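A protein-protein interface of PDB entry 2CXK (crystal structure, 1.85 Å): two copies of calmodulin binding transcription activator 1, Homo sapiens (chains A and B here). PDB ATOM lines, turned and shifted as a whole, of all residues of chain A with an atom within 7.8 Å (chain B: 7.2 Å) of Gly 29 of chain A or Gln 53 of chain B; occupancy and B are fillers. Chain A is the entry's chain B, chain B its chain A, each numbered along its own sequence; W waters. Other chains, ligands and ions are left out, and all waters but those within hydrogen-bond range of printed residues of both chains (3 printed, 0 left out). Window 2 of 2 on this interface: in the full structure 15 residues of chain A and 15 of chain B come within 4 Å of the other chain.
Gly 29 of chain A touches Gln 53 of chain B, and with the chains exchanged Gln 53 of chain A touches Gly 29 of chain B.
Gln 53 of chain A touches Gly 55 of chain B, and with the chains exchanged Gly 55 of chain A touches Gln 53 of chain B.
Val 56 of chain B touches its own counterpart, Val 56 of chain A.
Of the 9 pairs that touch across the chains among the printed residues, 5 have their exchanged pair printed and touching as well.
Hydrophobic or aromatic side chains of chain B within 4 Å of the printed part of chain A: Ile 52 and Val 56.
Of the 21 printed residues of chain A, 7 touch a printed residue of chain B.
Printed residues of chain A that touch a printed residue of chain B: Thr 10, Asp 11, Thr 28, Gly 29, Gln 53, Gly 55 and Val 56.
Hydrophobic or aromatic side chains of chain A within 4 Å of the printed part of chain B: Val 56.
Among the printed residues, 9 pairs touch across the chains.
Among the printed residues, no Asp or Glu carboxylate lies within 4 Å of a Lys or Arg side-chain nitrogen of the other chain.
Among the printed residues, pairs that only touch across the chains: Thr 28 of chain A with Val 56 of chain B (3.6 Å), Val 56 of chain A with Val 56 of chain B (3.7 Å), Asp 11 of chain A with Ile 52 of chain B (3.7 Å) and Thr 10 of chain A with Ile 52 of chain B (3.8 Å).
The side-chain amide nitrogen of Gln 53 of chain A is in hydrogen-bond range of the backbone carbonyl oxygen of Gly 29 of chain B (3.1 Å).
OG1 of Thr 10 of chain A sits at hydrogen-bond distance from OE1 of Gln 53 of chain B, at 2.7 Å.
NE2 of Gln 53 of chain B lies within hydrogen-bond range of O of Gly 29 of chain A.
The backbone carbonyl oxygen of Gly 55 of chain A sits at hydrogen-bond distance from the side-chain amide nitrogen of Gln 53 of chain B (3.5 Å).
The backbone carbonyl oxygen (O) of Gly 55 of chain B sits at hydrogen-bond distance from the side-chain amide nitrogen (NE2) of Gln 53 of chain A.
N of Gly 29 of chain B lies within hydrogen-bond range of O of Gly 55 of chain B.
The backbone carbonyl oxygen (O) of Trp 31 of chain B lies within hydrogen-bond range of the backbone NH (N) of Gly 55 of chain B (2.7 Å).
N of Thr 10 of chain A is in hydrogen-bond range of O of Thr 28 of chain A (2.8 Å).
OG1 of Thr 10 of chain A sits at hydrogen-bond distance from N of Gly 29 of chain A, at 3.4 Å.
N of Thr 28 of chain A lies within hydrogen-bond range of O of Asp 11 of chain A (2.9 Å).
The backbone carbonyl oxygen (O) of Gly 55 of chain A sits at hydrogen-bond distance from the backbone NH (N) of Gly 29 of chain A (3.1 Å).
Gly 29 of chain A touches just one residue of chain B: Gln 53 (3.0 Å).
Of chain A, only Thr 10, Gly 29 and Gly 55 come within 4 Å of Gln 53 of chain B.
Printed residues of chain A within 4 Å of Gly 29 of chain B: Gln 53.
Printed residues of chain B within 4 Å of Thr 28 of chain A: Val 56 (3.6 Å).
Of the printed residues of chain A, Gly 55 of chain B touches Gln 53 (3.5 Å).
Printed residues of chain A within 4 Å of Val 56 of chain B: Thr 28 (3.6 Å) and Val 56 (3.7 Å).
Printed residues of chain B within 4 Å of Gly 55 of chain A: Gln 53.
The nearest printed residue of chain B that does not touch Gly 55 of chain A is Val 56 of chain B (4.9 Å).
Water W1 lies within hydrogen-bond range of O of Pro 54 of chain B (2.6 Å), O of Pro 54 of chain A (2.7 Å) and NE2 of Gln 53 of chain B (2.9 Å).
Water W2 lies within hydrogen-bond range of the side-chain amide oxygen of Gln 53 of chain A (2.8 Å) and the backbone carbonyl oxygen of Gly 29 of chain B (3.5 Å).
Water W3 lies within hydrogen-bond range of OE1 of Gln 53 of chain B (2.9 Å) and O of Gly 29 of chain A (3.5 Å).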
ATOM      1  N   GLY A   7      -8.188  -3.592 -23.114  1.00  0.00           N
ATOM      2  CA  GLY A   7      -7.123  -4.576 -22.846  1.00  0.00           C
ATOM      3  C   GLY A   7      -6.238  -4.139 -21.697  1.00  0.00           C
ATOM      4  O   GLY A   7      -6.722  -3.690 -20.661  1.00  0.00           O
ATOM      5  N   MET A   8      -4.933  -4.261 -21.876  1.00  0.00           N
ATOM      6  CA  MET A   8      -4.016  -3.886 -20.819  1.00  0.00           C
ATOM      7  C   MET A   8      -3.028  -2.795 -21.175  1.00  0.00           C
ATOM      8  O   MET A   8      -2.622  -2.645 -22.325  1.00  0.00           O
ATOM      9  CB  MET A   8      -3.250  -5.110 -20.344  1.00  0.00           C
ATOM     10  CG  MET A   8      -4.102  -6.123 -19.607  1.00  0.00           C
ATOM     11  SD  MET A   8      -2.934  -7.417 -18.839  1.00  0.00           S
ATOM     12  CE  MET A   8      -2.382  -8.293 -20.469  1.00  0.00           C
ATOM     13  N   VAL A   9      -2.649  -2.035 -20.157  1.00  0.00           N
ATOM     14  CA  VAL A   9      -1.685  -0.964 -20.312  1.00  0.00           C
ATOM     15  C   VAL A   9      -0.351  -1.611 -20.643  1.00  0.00           C
ATOM     16  O   VAL A   9       0.100  -2.499 -19.920  1.00  0.00           O
ATOM     17  CB  VAL A   9      -1.544  -0.165 -19.000  1.00  0.00           C
ATOM     18  CG1 VAL A   9      -0.397   0.820 -19.114  1.00  0.00           C
ATOM     19  CG2 VAL A   9      -2.847   0.572 -18.698  1.00  0.00           C
ATOM     20  N   THR A  10       0.273  -1.187 -21.740  1.00  0.00           N
ATOM     21  CA  THR A  10       1.565  -1.751 -22.119  1.00  0.00           C
ATOM     22  C   THR A  10       2.722  -0.977 -21.495  1.00  0.00           C
ATOM     23  O   THR A  10       3.774  -1.548 -21.227  1.00  0.00           O
ATOM     24  CB  THR A  10       1.746  -1.804 -23.655  1.00  0.00           C
ATOM     25  OG1 THR A  10       1.418  -0.538 -24.230  1.00  0.00           O
ATOM     26  CG2 THR A  10       0.848  -2.875 -24.249  1.00  0.00           C
ATOM     27  N   ASP A  11       2.516   0.315 -21.260  1.00  0.00           N
ATOM     28  CA  ASP A  11       3.537   1.158 -20.636  1.00  0.00           C
ATOM     29  C   ASP A  11       2.936   2.517 -20.324  1.00  0.00           C
ATOM     30  O   ASP A  11       1.846   2.846 -20.785  1.00  0.00           O
ATOM     31  CB  ASP A  11       4.742   1.343 -21.566  1.00  0.00           C
ATOM     32  CG  ASP A  11       6.062   1.346 -20.816  1.00  0.00           C
ATOM     33  OD1 ASP A  11       6.092   1.807 -19.655  1.00  0.00           O
ATOM     34  OD2 ASP A  11       7.073   0.887 -21.391  1.00  0.00           O
ATOM     35  N   TYR A  12       3.651   3.309 -19.534  1.00  0.00           N
ATOM     36  CA  TYR A  12       3.198   4.645 -19.187  1.00  0.00           C
ATOM     37  C   TYR A  12       4.387   5.406 -18.627  1.00  0.00           C
ATOM     38  O   TYR A  12       5.286   4.812 -18.039  1.00  0.00           O
ATOM     39  CB  TYR A  12       2.038   4.583 -18.189  1.00  0.00           C
ATOM     40  CG  TYR A  12       2.309   3.832 -16.906  1.00  0.00           C
ATOM     41  CD1 TYR A  12       2.439   4.515 -15.697  1.00  0.00           C
ATOM     42  CD2 TYR A  12       2.378   2.440 -16.889  1.00  0.00           C
ATOM     43  CE1 TYR A  12       2.621   3.831 -14.495  1.00  0.00           C
ATOM     44  CE2 TYR A  12       2.561   1.739 -15.691  1.00  0.00           C
ATOM     45  CZ  TYR A  12       2.676   2.444 -14.500  1.00  0.00           C
ATOM     46  OH  TYR A  12       2.804   1.762 -13.307  1.00  0.00           O
ATOM     47  N   LEU A  26       1.866   9.818 -20.525  1.00  0.00           N
ATOM     48  CA  LEU A  26       1.484   9.100 -21.731  1.00  0.00           C
ATOM     49  C   LEU A  26       1.203   7.679 -21.278  1.00  0.00           C
ATOM     50  O   LEU A  26       1.955   7.122 -20.486  1.00  0.00           O
ATOM     51  CB  LEU A  26       2.617   9.092 -22.772  1.00  0.00           C
ATOM     52  CG  LEU A  26       2.986  10.439 -23.399  1.00  0.00           C
ATOM     53  CD1 LEU A  26       4.044  10.205 -24.461  1.00  0.00           C
ATOM     54  CD2 LEU A  26       1.750  11.117 -24.019  1.00  0.00           C
ATOM     55  N   ILE A  27       0.110   7.096 -21.763  1.00  0.00           N
ATOM     56  CA  ILE A  27      -0.247   5.734 -21.402  1.00  0.00           C
ATOM     57  C   ILE A  27      -0.536   4.985 -22.682  1.00  0.00           C
ATOM     58  O   ILE A  27      -1.463   5.342 -23.413  1.00  0.00           O
ATOM     59  CB  ILE A  27      -1.503   5.691 -20.504  1.00  0.00           C
ATOM     60  CG1 ILE A  27      -1.267   6.524 -19.248  1.00  0.00           C
ATOM     61  CG2 ILE A  27      -1.810   4.242 -20.123  1.00  0.00           C
ATOM     62  CD1 ILE A  27      -2.495   6.654 -18.350  1.00  0.00           C
ATOM     63  N   THR A  28       0.259   3.954 -22.956  1.00  0.00           N
ATOM     64  CA  THR A  28       0.104   3.171 -24.174  1.00  0.00           C
ATOM     65  C   THR A  28      -0.628   1.857 -23.941  1.00  0.00           C
ATOM     66  O   THR A  28      -0.581   1.276 -22.855  1.00  0.00           O
ATOM     67  CB  THR A  28       1.480   2.893 -24.837  1.00  0.00           C
ATOM     68  OG1 THR A  28       2.315   2.161 -23.934  1.00  0.00           O
ATOM     69  CG2 THR A  28       2.164   4.203 -25.195  1.00  0.00           C
ATOM     70  N   GLY A  29      -1.314   1.399 -24.978  1.00  0.00           N
ATOM     71  CA  GLY A  29      -2.076   0.175 -24.883  1.00  0.00           C
ATOM     72  C   GLY A  29      -2.875  -0.023 -26.154  1.00  0.00           C
ATOM     73  O   GLY A  29      -2.563   0.583 -27.172  1.00  0.00           O
ATOM     74  N   PRO A  30      -3.931  -0.847 -26.124  1.00  0.00           N
ATOM     75  CA  PRO A  30      -4.761  -1.110 -27.305  1.00  0.00           C
ATOM     76  C   PRO A  30      -5.848  -0.077 -27.624  1.00  0.00           C
ATOM     77  O   PRO A  30      -6.879  -0.427 -28.193  1.00  0.00           O
ATOM     78  CB  PRO A  30      -5.346  -2.478 -26.994  1.00  0.00           C
ATOM     79  CG  PRO A  30      -5.586  -2.374 -25.502  1.00  0.00           C
ATOM     80  CD  PRO A  30      -4.323  -1.711 -24.994  1.00  0.00           C
ATOM     81  N   TRP A  31      -5.611   1.186 -27.284  1.00  0.00           N
ATOM     82  CA  TRP A  31      -6.585   2.256 -27.526  1.00  0.00           C
ATOM     83  C   TRP A  31      -6.711   2.575 -29.023  1.00  0.00           C
ATOM     84  O   TRP A  31      -5.786   3.114 -29.626  1.00  0.00           O
ATOM     85  CB  TRP A  31      -6.170   3.531 -26.777  1.00  0.00           C
ATOM     86  CG  TRP A  31      -5.283   3.298 -25.565  1.00  0.00           C
ATOM     87  CD1 TRP A  31      -4.105   3.941 -25.281  1.00  0.00           C
ATOM     88  CD2 TRP A  31      -5.494   2.362 -24.496  1.00  0.00           C
ATOM     89  NE1 TRP A  31      -3.571   3.459 -24.108  1.00  0.00           N
ATOM     90  CE2 TRP A  31      -4.400   2.492 -23.604  1.00  0.00           C
ATOM     91  CE3 TRP A  31      -6.498   1.428 -24.205  1.00  0.00           C
ATOM     92  CZ2 TRP A  31      -4.281   1.720 -22.443  1.00  0.00           C
ATOM     93  CZ3 TRP A  31      -6.378   0.659 -23.047  1.00  0.00           C
ATOM     94  CH2 TRP A  31      -5.274   0.812 -22.181  1.00  0.00           C
ATOM     95  N   GLN A  32      -7.862   2.264 -29.615  1.00  0.00           N
ATOM     96  CA  GLN A  32      -8.079   2.509 -31.041  1.00  0.00           C
ATOM     97  C   GLN A  32      -9.258   3.440 -31.344  1.00  0.00           C
ATOM     98  O   GLN A  32      -9.272   4.122 -32.371  1.00  0.00           O
ATOM     99  CB  GLN A  32      -8.291   1.178 -31.764  1.00  0.00           C
ATOM    100  CG  GLN A  32      -7.156   0.169 -31.590  1.00  0.00           C
ATOM    101  CD  GLN A  32      -5.812   0.701 -32.068  1.00  0.00           C
ATOM    102  OE1 GLN A  32      -5.709   1.271 -33.155  1.00  0.00           O
ATOM    103  NE2 GLN A  32      -4.771   0.508 -31.259  1.00  0.00           N
ATOM    104  N   LEU A  51      -6.354  10.902 -27.549  1.00  0.00           N
ATOM    105  CA  LEU A  51      -5.663   9.868 -28.299  1.00  0.00           C
ATOM    106  C   LEU A  51      -4.701  10.589 -29.252  1.00  0.00           C
ATOM    107  O   LEU A  51      -5.114  11.117 -30.286  1.00  0.00           O
ATOM    108  CB  LEU A  51      -6.663   9.020 -29.089  1.00  0.00           C
ATOM    109  CG  LEU A  51      -6.119   7.742 -29.732  1.00  0.00           C
ATOM    110  CD1 LEU A  51      -5.778   6.722 -28.663  1.00  0.00           C
ATOM    111  CD2 LEU A  51      -7.157   7.176 -30.682  1.00  0.00           C
ATOM    112  N   GLN A  53      -2.405   9.296 -31.034  1.00  0.00           N
ATOM    113  CA  GLN A  53      -2.390   8.455 -32.219  1.00  0.00           C
ATOM    114  C   GLN A  53      -2.802   7.078 -31.716  1.00  0.00           C
ATOM    115  O   GLN A  53      -2.771   6.826 -30.512  1.00  0.00           O
ATOM    116  CB  GLN A  53      -0.988   8.401 -32.833  1.00  0.00           C
ATOM    117  CG  GLN A  53       0.081   7.825 -31.919  1.00  0.00           C
ATOM    118  CD  GLN A  53       1.442   7.793 -32.593  1.00  0.00           C
ATOM    119  OE1 GLN A  53       1.954   8.825 -33.027  1.00  0.00           O
ATOM    120  NE2 GLN A  53       2.029   6.608 -32.687  1.00  0.00           N
ATOM    121  N   PRO A  54      -3.189   6.168 -32.622  1.00  0.00           N
ATOM    122  CA  PRO A  54      -3.593   4.838 -32.166  1.00  0.00           C
ATOM    123  C   PRO A  54      -2.640   4.261 -31.125  1.00  0.00           C
ATOM    124  O   PRO A  54      -1.428   4.279 -31.310  1.00  0.00           O
ATOM    125  CB  PRO A  54      -3.605   4.022 -33.456  1.00  0.00           C
ATOM    126  CG  PRO A  54      -4.020   5.029 -34.475  1.00  0.00           C
ATOM    127  CD  PRO A  54      -3.185   6.236 -34.095  1.00  0.00           C
ATOM    128  N   GLY A  55      -3.209   3.775 -30.024  1.00  0.00           N
ATOM    129  CA  GLY A  55      -2.425   3.166 -28.961  1.00  0.00           C
ATOM    130  C   GLY A  55      -1.757   4.114 -27.982  1.00  0.00           C
ATOM    131  O   GLY A  55      -1.117   3.676 -27.023  1.00  0.00           O
ATOM    132  N   VAL A  56      -1.911   5.410 -28.200  1.00  0.00           N
ATOM    133  CA  VAL A  56      -1.271   6.384 -27.329  1.00  0.00           C
ATOM    134  C   VAL A  56      -2.212   7.431 -26.758  1.00  0.00           C
ATOM    135  O   VAL A  56      -2.795   8.223 -27.499  1.00  0.00           O
ATOM    136  CB  VAL A  56      -0.149   7.118 -28.078  1.00  0.00           C
ATOM    137  CG1 VAL A  56       0.526   8.131 -27.154  1.00  0.00           C
ATOM    138  CG2 VAL A  56       0.843   6.105 -28.617  1.00  0.00           C
ATOM    139  N   LEU A  57      -2.339   7.439 -25.436  1.00  0.00           N
ATOM    140  CA  LEU A  57      -3.186   8.413 -24.753  1.00  0.00           C
ATOM    141  C   LEU A  57      -2.357   9.390 -23.936  1.00  0.00           C
ATOM    142  O   LEU A  57      -1.372   9.008 -23.301  1.00  0.00           O
ATOM    143  CB  LEU A  57      -4.170   7.712 -23.817  1.00  0.00           C
ATOM    144  CG  LEU A  57      -5.370   7.012 -24.458  1.00  0.00           C
ATOM    145  CD1 LEU A  57      -6.087   6.174 -23.413  1.00  0.00           C
ATOM    146  CD2 LEU A  57      -6.305   8.059 -25.052  1.00  0.00           C
ATOM    147  N   VAL A  73      -7.428   3.334 -17.368  1.00  0.00           N
ATOM    148  CA  VAL A  73      -7.903   3.989 -18.578  1.00  0.00           C
ATOM    149  C   VAL A  73      -9.381   3.650 -18.732  1.00  0.00           C
ATOM    150  O   VAL A  73      -9.785   2.509 -18.508  1.00  0.00           O
ATOM    151  CB  VAL A  73      -7.164   3.480 -19.828  1.00  0.00           C
ATOM    152  CG1 VAL A  73      -7.766   4.101 -21.080  1.00  0.00           C
ATOM    153  CG2 VAL A  73      -5.688   3.821 -19.725  1.00  0.00           C
ATOM    154  N   SER A  81      -9.214  -0.909 -18.787  1.00  0.00           N
ATOM    155  CA  SER A  81      -7.871  -1.460 -18.641  1.00  0.00           C
ATOM    156  C   SER A  81      -7.637  -2.011 -17.252  1.00  0.00           C
ATOM    157  O   SER A  81      -8.503  -1.936 -16.382  1.00  0.00           O
ATOM    158  CB  SER A  81      -6.827  -0.373 -18.882  1.00  0.00           C
ATOM    159  OG  SER A  81      -6.812   0.531 -17.787  1.00  0.00           O
ATOM    160  N   GLY B  29       5.548   8.020 -32.431  1.00  0.00           N
ATOM    161  CA  GLY B  29       5.678   8.485 -33.790  1.00  0.00           C
ATOM    162  C   GLY B  29       5.284   7.377 -34.735  1.00  0.00           C
ATOM    163  O   GLY B  29       4.613   6.429 -34.331  1.00  0.00           O
ATOM    164  N   TRP B  31       6.906   4.833 -35.924  1.00  0.00           N
ATOM    165  CA  TRP B  31       7.789   3.664 -35.921  1.00  0.00           C
ATOM    166  C   TRP B  31       6.988   2.375 -36.080  1.00  0.00           C
ATOM    167  O   TRP B  31       6.073   2.110 -35.308  1.00  0.00           O
ATOM    168  CB  TRP B  31       8.608   3.591 -34.625  1.00  0.00           C
ATOM    169  CG  TRP B  31       8.621   4.860 -33.812  1.00  0.00           C
ATOM    170  CD1 TRP B  31       8.140   5.015 -32.540  1.00  0.00           C
ATOM    171  CD2 TRP B  31       9.139   6.138 -34.203  1.00  0.00           C
ATOM    172  NE1 TRP B  31       8.325   6.305 -32.117  1.00  0.00           N
ATOM    173  CE2 TRP B  31       8.934   7.019 -33.114  1.00  0.00           C
ATOM    174  CE3 TRP B  31       9.752   6.629 -35.364  1.00  0.00           C
ATOM    175  CZ2 TRP B  31       9.323   8.361 -33.152  1.00  0.00           C
ATOM    176  CZ3 TRP B  31      10.138   7.969 -35.401  1.00  0.00           C
ATOM    177  CH2 TRP B  31       9.921   8.818 -34.301  1.00  0.00           C
ATOM    178  N   GLN B  32       7.353   1.564 -37.070  1.00  0.00           N
ATOM    179  CA  GLN B  32       6.642   0.314 -37.328  1.00  0.00           C
ATOM    180  C   GLN B  32       7.556  -0.903 -37.462  1.00  0.00           C
ATOM    181  O   GLN B  32       7.151  -2.023 -37.143  1.00  0.00           O
ATOM    182  CB  GLN B  32       5.805   0.450 -38.604  1.00  0.00           C
ATOM    183  CG  GLN B  32       4.740   1.538 -38.558  1.00  0.00           C
ATOM    184  CD  GLN B  32       3.632   1.239 -37.559  1.00  0.00           C
ATOM    185  OE1 GLN B  32       3.055   0.148 -37.563  1.00  0.00           O
ATOM    186  NE2 GLN B  32       3.325   2.211 -36.701  1.00  0.00           N
ATOM    187  N   SER B  50      13.400   0.141 -27.499  1.00  0.00           N
ATOM    188  CA  SER B  50      12.570  -1.032 -27.757  1.00  0.00           C
ATOM    189  C   SER B  50      11.202  -0.612 -28.277  1.00  0.00           C
ATOM    190  O   SER B  50      10.593   0.324 -27.755  1.00  0.00           O
ATOM    191  CB  SER B  50      12.366  -1.844 -26.474  1.00  0.00           C
ATOM    192  OG  SER B  50      13.584  -2.353 -25.980  1.00  0.00           O
ATOM    193  N   LEU B  51      10.720  -1.300 -29.305  1.00  0.00           N
ATOM    194  CA  LEU B  51       9.410  -0.997 -29.852  1.00  0.00           C
ATOM    195  C   LEU B  51       8.376  -1.715 -28.981  1.00  0.00           C
ATOM    196  O   LEU B  51       8.137  -2.906 -29.150  1.00  0.00           O
ATOM    197  CB  LEU B  51       9.305  -1.492 -31.295  1.00  0.00           C
ATOM    198  CG  LEU B  51       7.978  -1.130 -31.969  1.00  0.00           C
ATOM    199  CD1 LEU B  51       7.949   0.372 -32.257  1.00  0.00           C
ATOM    200  CD2 LEU B  51       7.803  -1.945 -33.251  1.00  0.00           C
ATOM    201  N   ILE B  52       7.787  -0.981 -28.041  1.00  0.00           N
ATOM    202  CA  ILE B  52       6.781  -1.501 -27.115  1.00  0.00           C
ATOM    203  C   ILE B  52       5.591  -2.058 -27.886  1.00  0.00           C
ATOM    204  O   ILE B  52       5.028  -3.099 -27.552  1.00  0.00           O
ATOM    205  CB  ILE B  52       6.273  -0.370 -26.181  1.00  0.00           C
ATOM    206  CG1 ILE B  52       7.418   0.125 -25.290  1.00  0.00           C
ATOM    207  CG2 ILE B  52       5.077  -0.851 -25.370  1.00  0.00           C
ATOM    208  CD1 ILE B  52       8.093  -0.973 -24.480  1.00  0.00           C
ATOM    209  N   GLN B  53       5.205  -1.316 -28.910  1.00  0.00           N
ATOM    210  CA  GLN B  53       4.108  -1.677 -29.784  1.00  0.00           C
ATOM    211  C   GLN B  53       4.214  -0.692 -30.928  1.00  0.00           C
ATOM    212  O   GLN B  53       4.933   0.299 -30.832  1.00  0.00           O
ATOM    213  CB  GLN B  53       2.764  -1.535 -29.065  1.00  0.00           C
ATOM    214  CG  GLN B  53       2.454  -0.139 -28.575  1.00  0.00           C
ATOM    215  CD  GLN B  53       1.119  -0.081 -27.863  1.00  0.00           C
ATOM    216  OE1 GLN B  53       0.908  -0.769 -26.866  1.00  0.00           O
ATOM    217  NE2 GLN B  53       0.206   0.734 -28.376  1.00  0.00           N
ATOM    218  N   PRO B  54       3.513  -0.950 -32.037  1.00  0.00           N
ATOM    219  CA  PRO B  54       3.606  -0.018 -33.157  1.00  0.00           C
ATOM    220  C   PRO B  54       3.461   1.442 -32.744  1.00  0.00           C
ATOM    221  O   PRO B  54       2.508   1.812 -32.060  1.00  0.00           O
ATOM    222  CB  PRO B  54       2.475  -0.474 -34.076  1.00  0.00           C
ATOM    223  CG  PRO B  54       2.434  -1.948 -33.837  1.00  0.00           C
ATOM    224  CD  PRO B  54       2.569  -2.042 -32.335  1.00  0.00           C
ATOM    225  N   GLY B  55       4.430   2.258 -33.146  1.00  0.00           N
ATOM    226  CA  GLY B  55       4.389   3.676 -32.856  1.00  0.00           C
ATOM    227  C   GLY B  55       4.909   4.110 -31.502  1.00  0.00           C
ATOM    228  O   GLY B  55       4.919   5.306 -31.207  1.00  0.00           O
ATOM    229  N   VAL B  56       5.359   3.158 -30.688  1.00  0.00           N
ATOM    230  CA  VAL B  56       5.848   3.488 -29.352  1.00  0.00           C
ATOM    231  C   VAL B  56       7.220   2.920 -29.037  1.00  0.00           C
ATOM    232  O   VAL B  56       7.395   1.708 -28.975  1.00  0.00           O
ATOM    233  CB  VAL B  56       4.874   2.980 -28.279  1.00  0.00           C
ATOM    234  CG1 VAL B  56       5.405   3.308 -26.883  1.00  0.00           C
ATOM    235  CG2 VAL B  56       3.500   3.601 -28.510  1.00  0.00           C
ATOM    236  N   LEU B  57       8.190   3.806 -28.834  1.00  0.00           N
ATOM    237  CA  LEU B  57       9.544   3.387 -28.486  1.00  0.00           C
ATOM    238  C   LEU B  57       9.840   3.720 -27.026  1.00  0.00           C
ATOM    239  O   LEU B  57       9.406   4.756 -26.519  1.00  0.00           O
ATOM    240  CB  LEU B  57      10.570   4.106 -29.363  1.00  0.00           C
ATOM    241  CG  LEU B  57      10.670   3.561 -30.781  1.00  0.00           C
ATOM    242  CD1 LEU B  57      11.542   4.468 -31.648  1.00  0.00           C
ATOM    243  CD2 LEU B  57      11.235   2.163 -30.698  1.00  0.00           C
HETATM  244  O   HOH W   1       0.429   2.441 -30.717  1.00  0.00           O
HETATM  245  O   HOH W   2       2.392   8.725 -35.758  1.00  0.00           O
HETATM  246  O   HOH W   3      -1.275  -2.639 -27.248  1.00  0.00           O
